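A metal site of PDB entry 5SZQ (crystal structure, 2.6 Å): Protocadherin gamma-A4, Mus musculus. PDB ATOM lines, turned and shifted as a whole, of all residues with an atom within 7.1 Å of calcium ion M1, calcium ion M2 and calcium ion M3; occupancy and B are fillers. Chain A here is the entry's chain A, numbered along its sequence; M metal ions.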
ATOM      1  N   GLU A  16     -10.814  30.802  31.293  1.00  0.00           N
ATOM      2  CA  GLU A  16      -9.547  30.195  31.705  1.00  0.00           C
ATOM      3  C   GLU A  16      -8.326  30.931  31.167  1.00  0.00           C
ATOM      4  O   GLU A  16      -7.247  30.823  31.742  1.00  0.00           O
ATOM      5  CB  GLU A  16      -9.507  28.729  31.255  1.00  0.00           C
ATOM      6  CG  GLU A  16      -9.503  28.565  29.740  1.00  0.00           C
ATOM      7  CD  GLU A  16      -9.225  27.138  29.325  1.00  0.00           C
ATOM      8  OE1 GLU A  16      -8.600  26.404  30.113  1.00  0.00           O
ATOM      9  OE2 GLU A  16      -9.645  26.735  28.212  1.00  0.00           O
ATOM     10  N   ASN A  17      -8.487  31.701  30.089  1.00  0.00           N
ATOM     11  CA  ASN A  17      -7.367  32.358  29.430  1.00  0.00           C
ATOM     12  C   ASN A  17      -7.010  33.702  30.052  1.00  0.00           C
ATOM     13  O   ASN A  17      -6.311  34.497  29.409  1.00  0.00           O
ATOM     14  CB  ASN A  17      -7.662  32.552  27.941  1.00  0.00           C
ATOM     15  CG  ASN A  17      -8.736  33.602  27.695  1.00  0.00           C
ATOM     16  OD1 ASN A  17      -9.620  33.821  28.525  1.00  0.00           O
ATOM     17  ND2 ASN A  17      -8.672  34.272  26.542  1.00  0.00           N
ATOM     18  N   GLU A  69      -1.706  30.713  35.734  1.00  0.00           N
ATOM     19  CA  GLU A  69      -2.723  30.519  34.709  1.00  0.00           C
ATOM     20  C   GLU A  69      -3.697  29.415  35.106  1.00  0.00           C
ATOM     21  O   GLU A  69      -3.289  28.332  35.536  1.00  0.00           O
ATOM     22  CB  GLU A  69      -2.052  30.189  33.369  1.00  0.00           C
ATOM     23  CG  GLU A  69      -3.021  29.873  32.227  1.00  0.00           C
ATOM     24  CD  GLU A  69      -3.601  31.120  31.578  1.00  0.00           C
ATOM     25  OE1 GLU A  69      -3.600  32.191  32.227  1.00  0.00           O
ATOM     26  OE2 GLU A  69      -4.065  31.015  30.414  1.00  0.00           O
ATOM     27  N   LEU A  70      -4.987  29.715  34.962  1.00  0.00           N
ATOM     28  CA  LEU A  70      -6.035  28.768  35.300  1.00  0.00           C
ATOM     29  C   LEU A  70      -6.381  27.943  34.079  1.00  0.00           C
ATOM     30  O   LEU A  70      -6.726  28.487  33.018  1.00  0.00           O
ATOM     31  CB  LEU A  70      -7.281  29.497  35.815  1.00  0.00           C
ATOM     32  CG  LEU A  70      -7.050  30.591  36.872  1.00  0.00           C
ATOM     33  CD1 LEU A  70      -8.358  31.251  37.278  1.00  0.00           C
ATOM     34  CD2 LEU A  70      -6.346  30.025  38.094  1.00  0.00           C
ATOM     35  N   ASP A  71      -6.293  26.627  34.204  1.00  0.00           N
ATOM     36  CA  ASP A  71      -6.620  25.714  33.123  1.00  0.00           C
ATOM     37  C   ASP A  71      -7.966  25.083  33.461  1.00  0.00           C
ATOM     38  O   ASP A  71      -8.080  24.381  34.472  1.00  0.00           O
ATOM     39  CB  ASP A  71      -5.535  24.657  32.958  1.00  0.00           C
ATOM     40  CG  ASP A  71      -5.567  24.005  31.594  1.00  0.00           C
ATOM     41  OD1 ASP A  71      -5.724  24.732  30.591  1.00  0.00           O
ATOM     42  OD2 ASP A  71      -5.444  22.763  31.534  1.00  0.00           O
ATOM     43  N   TYR A  72      -8.983  25.358  32.634  1.00  0.00           N
ATOM     44  CA  TYR A  72     -10.290  24.746  32.852  1.00  0.00           C
ATOM     45  C   TYR A  72     -10.167  23.231  32.887  1.00  0.00           C
ATOM     46  O   TYR A  72     -10.827  22.560  33.692  1.00  0.00           O
ATOM     47  CB  TYR A  72     -11.276  25.178  31.762  1.00  0.00           C
ATOM     48  CG  TYR A  72     -12.686  24.612  31.908  1.00  0.00           C
ATOM     49  CD1 TYR A  72     -13.718  25.404  32.383  1.00  0.00           C
ATOM     50  CD2 TYR A  72     -12.983  23.300  31.550  1.00  0.00           C
ATOM     51  CE1 TYR A  72     -15.007  24.905  32.522  1.00  0.00           C
ATOM     52  CE2 TYR A  72     -14.261  22.791  31.680  1.00  0.00           C
ATOM     53  CZ  TYR A  72     -15.263  23.593  32.167  1.00  0.00           C
ATOM     54  OH  TYR A  72     -16.542  23.093  32.297  1.00  0.00           O
ATOM     55  N   GLU A  73      -9.333  22.678  32.013  1.00  0.00           N
ATOM     56  CA  GLU A  73      -9.122  21.234  31.957  1.00  0.00           C
ATOM     57  C   GLU A  73      -8.472  20.683  33.223  1.00  0.00           C
ATOM     58  O   GLU A  73      -8.489  19.466  33.422  1.00  0.00           O
ATOM     59  CB  GLU A  73      -8.270  20.881  30.734  1.00  0.00           C
ATOM     60  CG  GLU A  73      -9.000  21.027  29.407  1.00  0.00           C
ATOM     61  CD  GLU A  73      -9.288  22.465  29.035  1.00  0.00           C
ATOM     62  OE1 GLU A  73      -8.353  23.289  29.112  1.00  0.00           O
ATOM     63  OE2 GLU A  73     -10.441  22.773  28.678  1.00  0.00           O
ATOM     64  N   ASP A  74      -7.906  21.551  34.064  1.00  0.00           N
ATOM     65  CA  ASP A  74      -7.356  21.113  35.343  1.00  0.00           C
ATOM     66  C   ASP A  74      -8.413  21.168  36.446  1.00  0.00           C
ATOM     67  O   ASP A  74      -8.570  20.203  37.206  1.00  0.00           O
ATOM     68  CB  ASP A  74      -6.153  21.980  35.719  1.00  0.00           C
ATOM     69  CG  ASP A  74      -5.419  21.464  36.948  1.00  0.00           C
ATOM     70  OD1 ASP A  74      -5.314  20.222  37.118  1.00  0.00           O
ATOM     71  OD2 ASP A  74      -4.941  22.301  37.755  1.00  0.00           O
ATOM     72  N   LEU A 101     -14.422  29.412  33.179  1.00  0.00           N
ATOM     73  CA  LEU A 101     -15.143  29.114  31.953  1.00  0.00           C
ATOM     74  C   LEU A 101     -14.211  28.459  30.955  1.00  0.00           C
ATOM     75  O   LEU A 101     -12.987  28.641  30.980  1.00  0.00           O
ATOM     76  CB  LEU A 101     -15.737  30.396  31.350  1.00  0.00           C
ATOM     77  CG  LEU A 101     -16.633  31.217  32.286  1.00  0.00           C
ATOM     78  CD1 LEU A 101     -17.169  32.448  31.581  1.00  0.00           C
ATOM     79  CD2 LEU A 101     -17.768  30.372  32.860  1.00  0.00           C
ATOM     80  N   ASP A 102     -14.793  27.657  30.066  1.00  0.00           N
ATOM     81  CA  ASP A 102     -14.023  26.895  29.085  1.00  0.00           C
ATOM     82  C   ASP A 102     -13.741  27.756  27.861  1.00  0.00           C
ATOM     83  O   ASP A 102     -14.645  28.395  27.313  1.00  0.00           O
ATOM     84  CB  ASP A 102     -14.787  25.637  28.687  1.00  0.00           C
ATOM     85  CG  ASP A 102     -14.125  24.902  27.544  1.00  0.00           C
ATOM     86  OD1 ASP A 102     -14.845  24.224  26.776  1.00  0.00           O
ATOM     87  OD2 ASP A 102     -12.889  25.010  27.397  1.00  0.00           O
ATOM     88  N   VAL A 103     -12.475  27.768  27.442  1.00  0.00           N
ATOM     89  CA  VAL A 103     -12.044  28.426  26.218  1.00  0.00           C
ATOM     90  C   VAL A 103     -11.492  27.360  25.288  1.00  0.00           C
ATOM     91  O   VAL A 103     -10.721  26.493  25.726  1.00  0.00           O
ATOM     92  CB  VAL A 103     -10.991  29.517  26.491  1.00  0.00           C
ATOM     93  CG1 VAL A 103     -10.504  30.126  25.185  1.00  0.00           C
ATOM     94  CG2 VAL A 103     -11.561  30.590  27.399  1.00  0.00           C
ATOM     95  N   ASN A 104     -11.896  27.406  24.025  1.00  0.00           N
ATOM     96  CA  ASN A 104     -11.418  26.437  23.030  1.00  0.00           C
ATOM     97  C   ASN A 104      -9.957  26.747  22.720  1.00  0.00           C
ATOM     98  O   ASN A 104      -9.615  27.407  21.740  1.00  0.00           O
ATOM     99  CB  ASN A 104     -12.285  26.490  21.772  1.00  0.00           C
ATOM    100  CG  ASN A 104     -11.895  25.449  20.747  1.00  0.00           C
ATOM    101  OD1 ASN A 104     -11.258  24.454  21.076  1.00  0.00           O
ATOM    102  ND2 ASN A 104     -12.269  25.676  19.490  1.00  0.00           N
ATOM    103  N   ASP A 105      -9.075  26.236  23.578  1.00  0.00           N
ATOM    104  CA  ASP A 105      -7.638  26.429  23.427  1.00  0.00           C
ATOM    105  C   ASP A 105      -6.871  25.122  23.210  1.00  0.00           C
ATOM    106  O   ASP A 105      -5.644  25.120  23.293  1.00  0.00           O
ATOM    107  CB  ASP A 105      -7.061  27.170  24.643  1.00  0.00           C
ATOM    108  CG  ASP A 105      -7.278  26.405  25.943  1.00  0.00           C
ATOM    109  OD1 ASP A 105      -7.273  27.071  27.002  1.00  0.00           O
ATOM    110  OD2 ASP A 105      -7.448  25.170  25.910  1.00  0.00           O
ATOM    111  N   ASN A 106      -7.573  24.015  22.934  1.00  0.00           N
ATOM    112  CA  ASN A 106      -6.921  22.744  22.644  1.00  0.00           C
ATOM    113  C   ASN A 106      -7.489  22.196  21.341  1.00  0.00           C
ATOM    114  O   ASN A 106      -8.652  21.799  21.289  1.00  0.00           O
ATOM    115  CB  ASN A 106      -7.129  21.734  23.786  1.00  0.00           C
ATOM    116  CG  ASN A 106      -6.214  21.994  24.970  1.00  0.00           C
ATOM    117  OD1 ASN A 106      -5.195  22.680  24.854  1.00  0.00           O
ATOM    118  ND2 ASN A 106      -6.578  21.449  26.119  1.00  0.00           N
ATOM    119  N   ALA A 107      -6.666  22.190  20.286  1.00  0.00           N
ATOM    120  CA  ALA A 107      -7.089  21.585  19.040  1.00  0.00           C
ATOM    121  C   ALA A 107      -7.227  20.066  19.216  1.00  0.00           C
ATOM    122  O   ALA A 107      -6.546  19.478  20.065  1.00  0.00           O
ATOM    123  CB  ALA A 107      -6.098  21.902  17.929  1.00  0.00           C
ATOM    124  N   PRO A 108      -8.108  19.421  18.452  1.00  0.00           N
ATOM    125  CA  PRO A 108      -8.305  17.983  18.617  1.00  0.00           C
ATOM    126  C   PRO A 108      -7.038  17.194  18.340  1.00  0.00           C
ATOM    127  O   PRO A 108      -6.226  17.557  17.483  1.00  0.00           O
ATOM    128  CB  PRO A 108      -9.404  17.651  17.607  1.00  0.00           C
ATOM    129  CG  PRO A 108      -9.421  18.802  16.657  1.00  0.00           C
ATOM    130  CD  PRO A 108      -9.041  19.992  17.475  1.00  0.00           C
ATOM    131  N   ASP A 136     -10.476  15.107  22.255  1.00  0.00           N
ATOM    132  CA  ASP A 136     -10.289  16.540  22.483  1.00  0.00           C
ATOM    133  C   ASP A 136     -10.381  16.815  23.982  1.00  0.00           C
ATOM    134  O   ASP A 136     -11.290  16.307  24.653  1.00  0.00           O
ATOM    135  CB  ASP A 136     -11.326  17.363  21.716  1.00  0.00           C
ATOM    136  CG  ASP A 136     -11.011  18.854  21.717  1.00  0.00           C
ATOM    137  OD1 ASP A 136      -9.881  19.239  22.080  1.00  0.00           O
ATOM    138  OD2 ASP A 136     -11.906  19.647  21.327  1.00  0.00           O
ATOM    139  N   SER A 137      -9.450  17.618  24.493  1.00  0.00           N
ATOM    140  CA  SER A 137      -9.404  17.923  25.909  1.00  0.00           C
ATOM    141  C   SER A 137     -10.438  18.979  26.310  1.00  0.00           C
ATOM    142  O   SER A 137     -10.808  19.049  27.484  1.00  0.00           O
ATOM    143  CB  SER A 137      -7.995  18.396  26.295  1.00  0.00           C
ATOM    144  OG  SER A 137      -7.041  17.382  26.025  1.00  0.00           O
ATOM    145  N   ASP A 138     -10.899  19.787  25.367  1.00  0.00           N
ATOM    146  CA  ASP A 138     -11.857  20.836  25.694  1.00  0.00           C
ATOM    147  C   ASP A 138     -13.229  20.232  25.987  1.00  0.00           C
ATOM    148  O   ASP A 138     -13.493  19.050  25.741  1.00  0.00           O
ATOM    149  CB  ASP A 138     -11.942  21.873  24.578  1.00  0.00           C
ATOM    150  CG  ASP A 138     -10.669  22.683  24.430  1.00  0.00           C
ATOM    151  OD1 ASP A 138     -10.371  23.482  25.348  1.00  0.00           O
ATOM    152  OD2 ASP A 138      -9.980  22.530  23.399  1.00  0.00           O
ATOM    153  N   SER A 139     -14.124  21.066  26.509  1.00  0.00           N
ATOM    154  CA  SER A 139     -15.437  20.636  26.972  1.00  0.00           C
ATOM    155  C   SER A 139     -16.540  21.253  26.129  1.00  0.00           C
ATOM    156  O   SER A 139     -16.324  22.228  25.393  1.00  0.00           O
ATOM    157  CB  SER A 139     -15.636  21.011  28.444  1.00  0.00           C
ATOM    158  OG  SER A 139     -14.452  20.766  29.190  1.00  0.00           O
ATOM    159  N   GLU A 141     -19.304  22.051  23.291  1.00  0.00           N
ATOM    160  CA  GLU A 141     -19.143  22.081  21.840  1.00  0.00           C
ATOM    161  C   GLU A 141     -17.695  22.333  21.434  1.00  0.00           C
ATOM    162  O   GLU A 141     -17.312  21.976  20.317  1.00  0.00           O
ATOM    163  CB  GLU A 141     -20.057  23.135  21.214  1.00  0.00           C
ATOM    164  CG  GLU A 141     -21.505  22.694  21.063  1.00  0.00           C
ATOM    165  CD  GLU A 141     -22.323  23.657  20.220  1.00  0.00           C
ATOM    166  OE1 GLU A 141     -21.899  24.820  20.058  1.00  0.00           O
ATOM    167  OE2 GLU A 141     -23.381  23.237  19.705  1.00  0.00           O
ATOM    168  N   ASN A 142     -16.894  22.940  22.316  1.00  0.00           N
ATOM    169  CA  ASN A 142     -15.470  23.045  22.072  1.00  0.00           C
ATOM    170  C   ASN A 142     -14.780  21.687  22.054  1.00  0.00           C
ATOM    171  O   ASN A 142     -13.634  21.599  21.615  1.00  0.00           O
ATOM    172  CB  ASN A 142     -14.800  23.941  23.129  1.00  0.00           C
ATOM    173  CG  ASN A 142     -15.438  25.317  23.250  1.00  0.00           C
ATOM    174  OD1 ASN A 142     -16.147  25.772  22.350  1.00  0.00           O
ATOM    175  ND2 ASN A 142     -15.176  25.994  24.367  1.00  0.00           N
ATOM    176  N   GLY A 143     -15.458  20.636  22.530  1.00  0.00           N
ATOM    177  CA  GLY A 143     -14.870  19.322  22.662  1.00  0.00           C
ATOM    178  C   GLY A 143     -15.395  18.299  21.667  1.00  0.00           C
ATOM    179  O   GLY A 143     -14.711  17.309  21.385  1.00  0.00           O
ATOM    180  N   LEU A 144     -16.608  18.505  21.155  1.00  0.00           N
ATOM    181  CA  LEU A 144     -17.095  17.664  20.075  1.00  0.00           C
ATOM    182  C   LEU A 144     -16.236  17.862  18.834  1.00  0.00           C
ATOM    183  O   LEU A 144     -15.678  18.938  18.618  1.00  0.00           O
ATOM    184  CB  LEU A 144     -18.564  17.973  19.776  1.00  0.00           C
ATOM    185  CG  LEU A 144     -19.583  17.665  20.874  1.00  0.00           C
ATOM    186  CD1 LEU A 144     -20.996  17.905  20.363  1.00  0.00           C
ATOM    187  CD2 LEU A 144     -19.436  16.233  21.396  1.00  0.00           C
ATOM    188  N   ASP A 189     -12.979  21.160  14.958  1.00  0.00           N
ATOM    189  CA  ASP A 189     -13.634  21.463  16.221  1.00  0.00           C
ATOM    190  C   ASP A 189     -14.932  22.195  15.966  1.00  0.00           C
ATOM    191  O   ASP A 189     -15.071  22.945  14.992  1.00  0.00           O
ATOM    192  CB  ASP A 189     -12.710  22.309  17.101  1.00  0.00           C
ATOM    193  CG  ASP A 189     -13.121  22.322  18.538  1.00  0.00           C
ATOM    194  OD1 ASP A 189     -14.289  22.005  18.821  1.00  0.00           O
ATOM    195  OD2 ASP A 189     -12.270  22.655  19.388  1.00  0.00           O
ATOM    196  N   GLN A 190     -15.905  22.000  16.867  1.00  0.00           N
ATOM    197  CA  GLN A 190     -17.204  22.643  16.751  1.00  0.00           C
ATOM    198  C   GLN A 190     -17.279  23.967  17.513  1.00  0.00           C
ATOM    199  O   GLN A 190     -18.118  24.815  17.182  1.00  0.00           O
ATOM    200  CB  GLN A 190     -18.294  21.670  17.239  1.00  0.00           C
ATOM    201  CG  GLN A 190     -19.687  22.273  17.433  1.00  0.00           C
ATOM    202  CD  GLN A 190     -20.355  22.680  16.127  1.00  0.00           C
ATOM    203  OE1 GLN A 190     -20.183  22.024  15.102  1.00  0.00           O
ATOM    204  NE2 GLN A 190     -21.120  23.771  16.173  1.00  0.00           N
ATOM    205  N   GLY A 191     -16.409  24.180  18.496  1.00  0.00           N
ATOM    206  CA  GLY A 191     -16.456  25.414  19.268  1.00  0.00           C
ATOM    207  C   GLY A 191     -15.817  26.583  18.527  1.00  0.00           C
ATOM    208  O   GLY A 191     -14.794  26.436  17.852  1.00  0.00           O
ATOM    209  N   LEU A 195     -11.009  24.966  15.783  1.00  0.00           N
ATOM    210  CA  LEU A 195      -9.605  24.587  15.731  1.00  0.00           C
ATOM    211  C   LEU A 195      -9.475  23.239  15.047  1.00  0.00           C
ATOM    212  O   LEU A 195     -10.108  22.261  15.459  1.00  0.00           O
ATOM    213  CB  LEU A 195      -8.980  24.519  17.124  1.00  0.00           C
ATOM    214  CG  LEU A 195      -8.624  25.865  17.765  1.00  0.00           C
ATOM    215  CD1 LEU A 195      -7.873  25.646  19.060  1.00  0.00           C
ATOM    216  CD2 LEU A 195      -7.820  26.709  16.793  1.00  0.00           C
HETATM  217 CA    CA M   1      -6.844  25.221  28.640  1.00  0.00          CA
HETATM  218 CA    CA M   2      -9.951  24.577  27.476  1.00  0.00          CA
HETATM  219 CA    CA M   3     -11.092  22.002  21.086  1.00  0.00          CA
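OD2 of Asp 189 binds calcium ion M3 (2.2 Å).
The backbone carbonyl oxygen (O) of Asn 106 is bound to calcium ion M3, 2.5 Å away.
OD1 of Asn 104 binds calcium ion M3.
OD2 of Asp 136 binds calcium ion M3 (2.5 Å).
OD2 of Asp 138 is bound to calcium ion M3 (2.6 Å).
The backbone carbonyl oxygen (O) of Asn 142 is bound to calcium ion M3 (2.6 Å).
Calcium ion M3 has six donor atoms within binding distance.
Calcium ion M2 is bound by OE2 of Glu 73 (2.2 Å), OE2 of Glu 16 (2.3 Å), OD1 of Asp 138 (2.4 Å), OE1 of Glu 73 (2.6 Å) and O of Val 103 (2.7 Å).
Slightly farther from calcium ion M2 lies the side-chain carboxylate (OD2) of Asp 102 (3.0 Å).
Slightly farther from calcium ion M2 lies the side-chain carboxylate (OD2) of Asp 105 (3.0 Å).
Four residues have an atom within 4 Å of calcium ion M1: Glu 16, Asp 71, Glu 73 and Asp 105.
The nearest printed residue that does not touch calcium ion M1 is Tyr 72 (4.5 Å).
Calcium ion M1 is bound by OD1 of Asp 71 (2.3 Å), OE1 of Glu 73 (2.5 Å), OD1 of Asp 105 (2.5 Å), OE1 of Glu 16 (2.6 Å) and OD2 of Asp 105 (2.8 Å).
Within 4 Å of calcium ion M2: Glu 16, Glu 73, Asp 102, Val 103, Asp 105 and Asp 138.
The nearest printed residue that does not touch calcium ion M2 is Tyr 72 (4.5 Å).
The side-chain amide nitrogen (ND2) of Asn 142 lies within hydrogen-bond range of the side-chain carboxylate (OD1) of Asp 102 (3.0 Å).
O of Glu 16 sits close to O of Leu 70.
The backbone NH of Glu 16 is in hydrogen-bond range of the backbone carbonyl oxygen of Leu 101 (3.1 Å).
The side-chain carboxylate of Glu 16 lies close to the backbone NH of Tyr 72, 2.8 Å away.
N of Ser 139 sits at hydrogen-bond distance from OD1 of Asp 102, at 3.3 Å.
The side-chain carboxylate (OD1) of Asp 189 sits at hydrogen-bond distance from the backbone NH (N) of Gly 191.
ND2 of Asn 104 sits at hydrogen-bond distance from O of Gly 191.
N of Asp 189 sits close to O of Leu 195, 3.1 Å away.
Six residues have an atom within 4 Å of calcium ion M3: Asn 104, Asn 106, Asp 136, Asp 138, Asn 142 and Asp 189.
The nearest printed residue that does not touch calcium ion M3 is Ala 107 (4.5 Å).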
